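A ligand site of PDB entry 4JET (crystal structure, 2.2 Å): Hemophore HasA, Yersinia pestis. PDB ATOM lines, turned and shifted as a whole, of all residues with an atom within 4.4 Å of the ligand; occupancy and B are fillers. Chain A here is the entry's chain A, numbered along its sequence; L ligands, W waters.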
ATOM      1  N   ASP A  31      -6.017 -13.060  -7.153  1.00  0.00           N
ATOM      2  CA  ASP A  31      -4.579 -12.882  -7.343  1.00  0.00           C
ATOM      3  C   ASP A  31      -4.266 -11.992  -8.549  1.00  0.00           C
ATOM      4  O   ASP A  31      -3.214 -11.349  -8.567  1.00  0.00           O
ATOM      5  CB  ASP A  31      -3.888 -14.260  -7.412  1.00  0.00           C
ATOM      6  CG  ASP A  31      -3.861 -14.967  -6.053  1.00  0.00           C
ATOM      7  OD1 ASP A  31      -4.129 -14.318  -5.008  1.00  0.00           O
ATOM      8  OD2 ASP A  31      -3.562 -16.181  -6.001  1.00  0.00           O
ATOM      9  N   ARG A  40     -10.384  -9.176   0.151  1.00  0.00           N
ATOM     10  CA  ARG A  40     -10.022 -10.475   0.721  1.00  0.00           C
ATOM     11  C   ARG A  40     -11.157 -11.090   1.511  1.00  0.00           C
ATOM     12  O   ARG A  40     -11.027 -12.229   1.944  1.00  0.00           O
ATOM     13  CB  ARG A  40      -8.826 -10.277   1.664  1.00  0.00           C
ATOM     14  CG  ARG A  40      -7.685  -9.517   1.033  1.00  0.00           C
ATOM     15  CD  ARG A  40      -6.483 -10.439   0.920  1.00  0.00           C
ATOM     16  NE  ARG A  40      -5.298  -9.726   0.431  1.00  0.00           N
ATOM     17  CZ  ARG A  40      -4.240 -10.342  -0.066  1.00  0.00           C
ATOM     18  NH1 ARG A  40      -4.212 -11.676  -0.133  1.00  0.00           N
ATOM     19  NH2 ARG A  40      -3.217  -9.624  -0.533  1.00  0.00           N
ATOM     20  N   GLY A  41     -12.243 -10.365   1.706  1.00  0.00           N
ATOM     21  CA  GLY A  41     -13.357 -10.862   2.483  1.00  0.00           C
ATOM     22  C   GLY A  41     -13.367 -10.287   3.876  1.00  0.00           C
ATOM     23  O   GLY A  41     -12.415  -9.642   4.333  1.00  0.00           O
ATOM     24  N   SER A  42     -14.458 -10.537   4.577  1.00  0.00           N
ATOM     25  CA  SER A  42     -14.706  -9.926   5.875  1.00  0.00           C
ATOM     26  C   SER A  42     -15.418 -10.972   6.727  1.00  0.00           C
ATOM     27  O   SER A  42     -16.449 -11.506   6.317  1.00  0.00           O
ATOM     28  CB  SER A  42     -15.573  -8.654   5.735  1.00  0.00           C
ATOM     29  OG  SER A  42     -15.747  -8.029   6.997  1.00  0.00           O
ATOM     30  N   PHE A  43     -14.852 -11.247   7.895  1.00  0.00           N
ATOM     31  CA  PHE A  43     -15.453 -12.117   8.884  1.00  0.00           C
ATOM     32  C   PHE A  43     -16.267 -11.283   9.833  1.00  0.00           C
ATOM     33  O   PHE A  43     -15.884 -10.162  10.138  1.00  0.00           O
ATOM     34  CB  PHE A  43     -14.375 -12.808   9.705  1.00  0.00           C
ATOM     35  CG  PHE A  43     -13.736 -13.947   9.020  1.00  0.00           C
ATOM     36  CD1 PHE A  43     -14.352 -15.169   8.997  1.00  0.00           C
ATOM     37  CD2 PHE A  43     -12.545 -13.804   8.391  1.00  0.00           C
ATOM     38  CE1 PHE A  43     -13.776 -16.237   8.364  1.00  0.00           C
ATOM     39  CE2 PHE A  43     -11.958 -14.879   7.752  1.00  0.00           C
ATOM     40  CZ  PHE A  43     -12.563 -16.088   7.746  1.00  0.00           C
ATOM     41  N   LEU A  49     -10.966 -10.719  13.565  1.00  0.00           N
ATOM     42  CA  LEU A  49     -10.604 -10.449  12.187  1.00  0.00           C
ATOM     43  C   LEU A  49     -10.558 -11.691  11.311  1.00  0.00           C
ATOM     44  O   LEU A  49     -10.914 -11.608  10.129  1.00  0.00           O
ATOM     45  CB  LEU A  49      -9.248  -9.726  12.152  1.00  0.00           C
ATOM     46  CG  LEU A  49      -8.792  -9.132  10.818  1.00  0.00           C
ATOM     47  CD1 LEU A  49      -9.679  -7.946  10.378  1.00  0.00           C
ATOM     48  CD2 LEU A  49      -7.322  -8.704  10.899  1.00  0.00           C
ATOM     49  N   PHE A  50     -10.167 -12.857  11.864  1.00  0.00           N
ATOM     50  CA  PHE A  50      -9.824 -14.042  11.093  1.00  0.00           C
ATOM     51  C   PHE A  50     -10.684 -15.247  11.446  1.00  0.00           C
ATOM     52  O   PHE A  50     -10.356 -16.361  11.049  1.00  0.00           O
ATOM     53  CB  PHE A  50      -8.346 -14.415  11.250  1.00  0.00           C
ATOM     54  CG  PHE A  50      -7.403 -13.374  10.715  1.00  0.00           C
ATOM     55  CD1 PHE A  50      -7.559 -12.863   9.445  1.00  0.00           C
ATOM     56  CD2 PHE A  50      -6.358 -12.886  11.511  1.00  0.00           C
ATOM     57  CE1 PHE A  50      -6.689 -11.892   8.957  1.00  0.00           C
ATOM     58  CE2 PHE A  50      -5.458 -11.919  11.012  1.00  0.00           C
ATOM     59  CZ  PHE A  50      -5.632 -11.424   9.748  1.00  0.00           C
ATOM     60  N   TYR A  55     -18.646 -15.248   6.650  1.00  0.00           N
ATOM     61  CA  TYR A  55     -17.548 -14.803   5.806  1.00  0.00           C
ATOM     62  C   TYR A  55     -18.149 -14.337   4.480  1.00  0.00           C
ATOM     63  O   TYR A  55     -18.815 -15.118   3.790  1.00  0.00           O
ATOM     64  CB  TYR A  55     -16.491 -15.898   5.604  1.00  0.00           C
ATOM     65  CG  TYR A  55     -15.407 -15.517   4.622  1.00  0.00           C
ATOM     66  CD1 TYR A  55     -14.405 -14.586   4.961  1.00  0.00           C
ATOM     67  CD2 TYR A  55     -15.369 -16.066   3.350  1.00  0.00           C
ATOM     68  CE1 TYR A  55     -13.435 -14.191   4.044  1.00  0.00           C
ATOM     69  CE2 TYR A  55     -14.396 -15.701   2.424  1.00  0.00           C
ATOM     70  CZ  TYR A  55     -13.435 -14.770   2.762  1.00  0.00           C
ATOM     71  OH  TYR A  55     -12.484 -14.428   1.815  1.00  0.00           O
ATOM     72  N   TYR A  75      -9.766 -19.016   9.886  1.00  0.00           N
ATOM     73  CA  TYR A  75      -8.735 -18.760   8.909  1.00  0.00           C
ATOM     74  C   TYR A  75      -7.425 -18.541   9.647  1.00  0.00           C
ATOM     75  O   TYR A  75      -7.329 -17.642  10.463  1.00  0.00           O
ATOM     76  CB  TYR A  75      -9.060 -17.493   8.121  1.00  0.00           C
ATOM     77  CG  TYR A  75      -7.962 -17.004   7.195  1.00  0.00           C
ATOM     78  CD1 TYR A  75      -7.444 -17.826   6.200  1.00  0.00           C
ATOM     79  CD2 TYR A  75      -7.469 -15.689   7.290  1.00  0.00           C
ATOM     80  CE1 TYR A  75      -6.464 -17.369   5.334  1.00  0.00           C
ATOM     81  CE2 TYR A  75      -6.492 -15.210   6.427  1.00  0.00           C
ATOM     82  CZ  TYR A  75      -5.999 -16.064   5.443  1.00  0.00           C
ATOM     83  OH  TYR A  75      -5.050 -15.606   4.574  1.00  0.00           O
ATOM     84  N   PHE A  77      -4.559 -17.421   8.622  1.00  0.00           N
ATOM     85  CA  PHE A  77      -3.676 -16.354   8.171  1.00  0.00           C
ATOM     86  C   PHE A  77      -2.239 -16.877   7.978  1.00  0.00           C
ATOM     87  O   PHE A  77      -2.056 -18.010   7.497  1.00  0.00           O
ATOM     88  CB  PHE A  77      -3.792 -15.191   9.160  1.00  0.00           C
ATOM     89  CG  PHE A  77      -3.156 -13.904   8.715  1.00  0.00           C
ATOM     90  CD1 PHE A  77      -3.359 -13.414   7.456  1.00  0.00           C
ATOM     91  CD2 PHE A  77      -2.369 -13.171   9.586  1.00  0.00           C
ATOM     92  CE1 PHE A  77      -2.794 -12.219   7.055  1.00  0.00           C
ATOM     93  CE2 PHE A  77      -1.812 -11.975   9.200  1.00  0.00           C
ATOM     94  CZ  PHE A  77      -2.014 -11.493   7.936  1.00  0.00           C
ATOM     95  N   MET A  78      -1.186 -16.113   8.351  1.00  0.00           N
ATOM     96  CA  MET A  78       0.193 -16.545   8.075  1.00  0.00           C
ATOM     97  C   MET A  78       0.611 -17.652   9.057  1.00  0.00           C
ATOM     98  O   MET A  78       0.207 -17.610  10.224  1.00  0.00           O
ATOM     99  CB  MET A  78       1.148 -15.370   8.233  1.00  0.00           C
ATOM    100  CG  MET A  78       0.735 -14.185   7.402  1.00  0.00           C
ATOM    101  SD  MET A  78       1.475 -12.662   7.965  1.00  0.00           S
ATOM    102  CE  MET A  78       3.208 -13.071   7.793  1.00  0.00           C
ATOM    103  N   HIS A  81      -2.290 -20.011   5.754  1.00  0.00           N
ATOM    104  CA  HIS A  81      -3.496 -19.408   5.181  1.00  0.00           C
ATOM    105  C   HIS A  81      -4.565 -20.446   4.837  1.00  0.00           C
ATOM    106  O   HIS A  81      -4.974 -20.593   3.688  1.00  0.00           O
ATOM    107  CB  HIS A  81      -3.145 -18.596   3.949  1.00  0.00           C
ATOM    108  CG  HIS A  81      -2.115 -17.552   4.196  1.00  0.00           C
ATOM    109  ND1 HIS A  81      -2.421 -16.264   4.568  1.00  0.00           N
ATOM    110  CD2 HIS A  81      -0.754 -17.615   4.124  1.00  0.00           C
ATOM    111  CE1 HIS A  81      -1.307 -15.568   4.706  1.00  0.00           C
ATOM    112  NE2 HIS A  81      -0.286 -16.362   4.433  1.00  0.00           N
ATOM    113  N   PHE A  83      -8.358 -21.910   5.392  1.00  0.00           N
ATOM    114  CA  PHE A  83      -9.734 -21.696   5.792  1.00  0.00           C
ATOM    115  C   PHE A  83     -10.298 -23.045   6.188  1.00  0.00           C
ATOM    116  O   PHE A  83     -10.280 -23.993   5.395  1.00  0.00           O
ATOM    117  CB  PHE A  83     -10.455 -21.115   4.576  1.00  0.00           C
ATOM    118  CG  PHE A  83     -11.841 -20.594   4.828  1.00  0.00           C
ATOM    119  CD1 PHE A  83     -12.110 -19.790   5.877  1.00  0.00           C
ATOM    120  CD2 PHE A  83     -12.850 -20.850   3.906  1.00  0.00           C
ATOM    121  CE1 PHE A  83     -13.387 -19.255   6.059  1.00  0.00           C
ATOM    122  CE2 PHE A  83     -14.124 -20.328   4.090  1.00  0.00           C
ATOM    123  CZ  PHE A  83     -14.381 -19.521   5.152  1.00  0.00           C
ATOM    124  N   HIS A 135      -4.099 -27.512   2.824  1.00  0.00           N
ATOM    125  CA  HIS A 135      -4.839 -27.019   1.666  1.00  0.00           C
ATOM    126  C   HIS A 135      -5.595 -28.105   0.906  1.00  0.00           C
ATOM    127  O   HIS A 135      -6.192 -27.796  -0.119  1.00  0.00           O
ATOM    128  CB  HIS A 135      -3.906 -26.281   0.706  1.00  0.00           C
ATOM    129  CG  HIS A 135      -3.490 -24.937   1.200  1.00  0.00           C
ATOM    130  ND1 HIS A 135      -2.864 -24.014   0.401  1.00  0.00           N
ATOM    131  CD2 HIS A 135      -3.615 -24.355   2.420  1.00  0.00           C
ATOM    132  CE1 HIS A 135      -2.623 -22.921   1.097  1.00  0.00           C
ATOM    133  NE2 HIS A 135      -3.073 -23.108   2.332  1.00  0.00           N
ATOM    134  N   HIS A 140     -11.343 -25.586   2.385  1.00  0.00           N
ATOM    135  CA  HIS A 140     -10.306 -24.668   1.927  1.00  0.00           C
ATOM    136  C   HIS A 140     -10.242 -24.644   0.403  1.00  0.00           C
ATOM    137  O   HIS A 140     -10.273 -23.582  -0.233  1.00  0.00           O
ATOM    138  CB  HIS A 140      -8.913 -25.011   2.499  1.00  0.00           C
ATOM    139  CG  HIS A 140      -7.838 -24.176   1.899  1.00  0.00           C
ATOM    140  ND1 HIS A 140      -7.442 -22.980   2.449  1.00  0.00           N
ATOM    141  CD2 HIS A 140      -7.181 -24.278   0.721  1.00  0.00           C
ATOM    142  CE1 HIS A 140      -6.548 -22.400   1.665  1.00  0.00           C
ATOM    143  NE2 HIS A 140      -6.388 -23.173   0.604  1.00  0.00           N
ATOM    144  N   VAL A 143     -13.465 -23.015  -1.445  1.00  0.00           N
ATOM    145  CA  VAL A 143     -13.629 -21.568  -1.301  1.00  0.00           C
ATOM    146  C   VAL A 143     -12.482 -20.828  -1.973  1.00  0.00           C
ATOM    147  O   VAL A 143     -12.687 -19.793  -2.628  1.00  0.00           O
ATOM    148  CB  VAL A 143     -13.770 -21.198   0.175  1.00  0.00           C
ATOM    149  CG1 VAL A 143     -13.743 -19.723   0.322  1.00  0.00           C
ATOM    150  CG2 VAL A 143     -15.023 -21.763   0.746  1.00  0.00           C
ATOM    151  N   ARG A 144     -11.255 -21.325  -1.768  1.00  0.00           N
ATOM    152  CA  ARG A 144     -10.069 -20.715  -2.389  1.00  0.00           C
ATOM    153  C   ARG A 144     -10.172 -20.735  -3.909  1.00  0.00           C
ATOM    154  O   ARG A 144      -9.882 -19.739  -4.579  1.00  0.00           O
ATOM    155  CB  ARG A 144      -8.794 -21.443  -1.933  1.00  0.00           C
ATOM    156  CG  ARG A 144      -7.506 -20.792  -2.468  1.00  0.00           C
ATOM    157  CD  ARG A 144      -7.479 -19.284  -2.175  1.00  0.00           C
ATOM    158  NE  ARG A 144      -6.240 -18.660  -2.603  1.00  0.00           N
ATOM    159  CZ  ARG A 144      -6.025 -17.347  -2.569  1.00  0.00           C
ATOM    160  NH1 ARG A 144      -6.951 -16.523  -2.141  1.00  0.00           N
ATOM    161  NH2 ARG A 144      -4.854 -16.853  -2.967  1.00  0.00           N
ATOM    162  N   MET A 147     -12.423 -17.853  -4.808  1.00  0.00           N
ATOM    163  CA  MET A 147     -11.745 -16.580  -4.680  1.00  0.00           C
ATOM    164  C   MET A 147     -10.856 -16.347  -5.895  1.00  0.00           C
ATOM    165  O   MET A 147     -10.633 -15.190  -6.289  1.00  0.00           O
ATOM    166  CB  MET A 147     -10.863 -16.601  -3.428  1.00  0.00           C
ATOM    167  CG  MET A 147     -11.583 -16.604  -2.117  1.00  0.00           C
ATOM    168  SD  MET A 147     -10.392 -16.676  -0.725  1.00  0.00           S
ATOM    169  CE  MET A 147      -9.800 -15.011  -0.767  1.00  0.00           C
HETATM  170  C1  LIG L   1      -2.558 -14.552   1.678  1.00  0.00           C
HETATM  171  C2  LIG L   1      -5.311 -11.413   4.060  1.00  0.00           C
HETATM  172  C3  LIG L   1      -8.904 -14.653   3.819  1.00  0.00           C
HETATM  173  C4  LIG L   1      -6.275 -17.813   1.356  1.00  0.00           C
HETATM  174  C5  LIG L   1      -2.946 -13.426   2.321  1.00  0.00           C
HETATM  175  C6  LIG L   1      -2.189 -12.194   2.511  1.00  0.00           C
HETATM  176  C7  LIG L   1      -2.966 -11.348   3.160  1.00  0.00           C
HETATM  177  C8  LIG L   1      -4.248 -11.977   3.399  1.00  0.00           C
HETATM  178  C9  LIG L   1      -2.630  -9.923   3.621  1.00  0.00           C
HETATM  179  C10 LIG L   1      -0.735 -11.925   2.081  1.00  0.00           C
HETATM  180  C11 LIG L   1       0.130 -12.780   3.010  1.00  0.00           C
HETATM  181  C12 LIG L   1       1.592 -12.375   2.966  1.00  0.00           C
HETATM  182  O1  LIG L   1       1.945 -11.320   2.355  1.00  0.00           O
HETATM  183  O2  LIG L   1       2.421 -13.121   3.558  1.00  0.00           O
HETATM  184  C13 LIG L   1      -6.493 -12.047   4.219  1.00  0.00           C
HETATM  185  C14 LIG L   1      -7.600 -11.484   4.917  1.00  0.00           C
HETATM  186  C15 LIG L   1      -8.591 -12.380   4.845  1.00  0.00           C
HETATM  187  C16 LIG L   1      -8.127 -13.534   4.087  1.00  0.00           C
HETATM  188  C17 LIG L   1      -7.555 -10.097   5.618  1.00  0.00           C
HETATM  189  C18 LIG L   1     -10.007 -12.310   5.420  1.00  0.00           C
HETATM  190  C19 LIG L   1     -10.504 -11.259   6.080  1.00  0.00           C
HETATM  191  C20 LIG L   1      -8.542 -15.781   3.143  1.00  0.00           C
HETATM  192  C21 LIG L   1      -9.382 -16.946   2.886  1.00  0.00           C
HETATM  193  C22 LIG L   1      -8.609 -17.837   2.232  1.00  0.00           C
HETATM  194  C23 LIG L   1      -7.332 -17.237   2.000  1.00  0.00           C
HETATM  195  C24 LIG L   1     -10.854 -17.090   3.381  1.00  0.00           C
HETATM  196  C25 LIG L   1      -8.935 -19.194   1.654  1.00  0.00           C
HETATM  197  C26 LIG L   1     -10.180 -19.433   1.267  1.00  0.00           C
HETATM  198  C27 LIG L   1      -5.038 -17.204   1.253  1.00  0.00           C
HETATM  199  C28 LIG L   1      -3.915 -17.821   0.601  1.00  0.00           C
HETATM  200  C29 LIG L   1      -2.795 -16.804   0.693  1.00  0.00           C
HETATM  201  C30 LIG L   1      -3.328 -15.664   1.399  1.00  0.00           C
HETATM  202  C31 LIG L   1      -3.863 -19.238  -0.036  1.00  0.00           C
HETATM  203  C32 LIG L   1      -1.367 -16.957   0.171  1.00  0.00           C
HETATM  204  C33 LIG L   1      -1.382 -16.800  -1.340  1.00  0.00           C
HETATM  205  C34 LIG L   1      -1.338 -18.190  -1.944  1.00  0.00           C
HETATM  206  O3  LIG L   1      -2.222 -18.458  -2.809  1.00  0.00           O
HETATM  207  O4  LIG L   1      -0.447 -19.008  -1.529  1.00  0.00           O
HETATM  208  N1  LIG L   1      -4.198 -13.234   2.883  1.00  0.00           N
HETATM  209  N2  LIG L   1      -6.821 -13.313   3.703  1.00  0.00           N
HETATM  210  N3  LIG L   1      -7.334 -16.016   2.589  1.00  0.00           N
HETATM  211  N4  LIG L   1      -4.675 -15.938   1.735  1.00  0.00           N
HETATM  212 FE1  LIG L   1      -5.678 -14.660   2.738  1.00  0.00          FE
HETATM  213  O   HOH W   1       4.871 -12.268   4.188  1.00  0.00           O
HETATM  214  O   HOH W   2       2.139 -15.238   4.682  1.00  0.00           O
HETATM  215  O   HOH W   3      -4.284 -20.553  -3.307  1.00  0.00           O
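The guanidinium group (NH2) of Arg 144 is in salt-bridge range of an oxygen (O3) of the ligand, 3.1 Å away. The side-chain hydroxyl (OH) of Tyr 75 is bound to an iron atom (FE1) of the ligand (2.2 Å).
The backbone carbonyl oxygen (O) of Arg 40 is in hydrogen-bond range of the side-chain hydroxyl (OH) of Tyr 55 (2.6 Å). The side-chain sulfur of Met 147 lies close to the guanidinium group of Arg 144 (3.7 Å). The backbone NH (N) of Tyr 75 sits at hydrogen-bond distance from the backbone carbonyl oxygen (O) of Phe 50, 3.0 Å away. The backbone carbonyl oxygen (O) of His 81 lies within hydrogen-bond range of a ring nitrogen (NE2) of His 135, at 3.4 Å. N of Phe 83 lies within hydrogen-bond range of ND1 of His 140, at 3.3 Å. The backbone carbonyl oxygen (O) of Phe 77 sits close to a ring nitrogen (ND1) of His 81, 3.4 Å away. ND1 of His 81 lies close to OH of Tyr 75 (2.7 Å). The side-chain carboxylate (OD1) of Asp 31 is in salt-bridge range of the guanidinium group (NH2) of Arg 144, 3.3 Å away.
The guanidinium group (NH1) of Arg 40 lies close to a nitrogen (N1) of the ligand. O of Gly 41 touches C19 of the ligand, at 3.1 Å. CE2 of Phe 43 touches C18 of the ligand (3.98 Å). Phe 50 touches the ligand (CE1 to C17, 3.9 Å). Tyr 55 touches the ligand. Phe 77 touches the ligand (CE1 to C8, 3.9 Å). His 81 touches the ligand. CB of Phe 83 touches C26 of the ligand (3.7 Å). CE1 of His 140 touches C25 of the ligand, at 3.997 Å. CG1 of Val 143 touches C26 of the ligand, 3.7 Å away. Met 147 touches the ligand (SD to C26, 3.4 Å). Hydrophobic or aromatic side chains within 4 Å of the ligand: Phe 43, Phe 50, Tyr 55, Tyr 75, Phe 77, His 81, Phe 83, His 140, Val 143 and Met 147.
Water W2 lies within hydrogen-bond range of an oxygen (O2) of the ligand and a ring nitrogen (NE2) of His 81. Water W3 bridges NE of Arg 144 (2.8 Å) and O3 of the ligand (3.0 Å).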
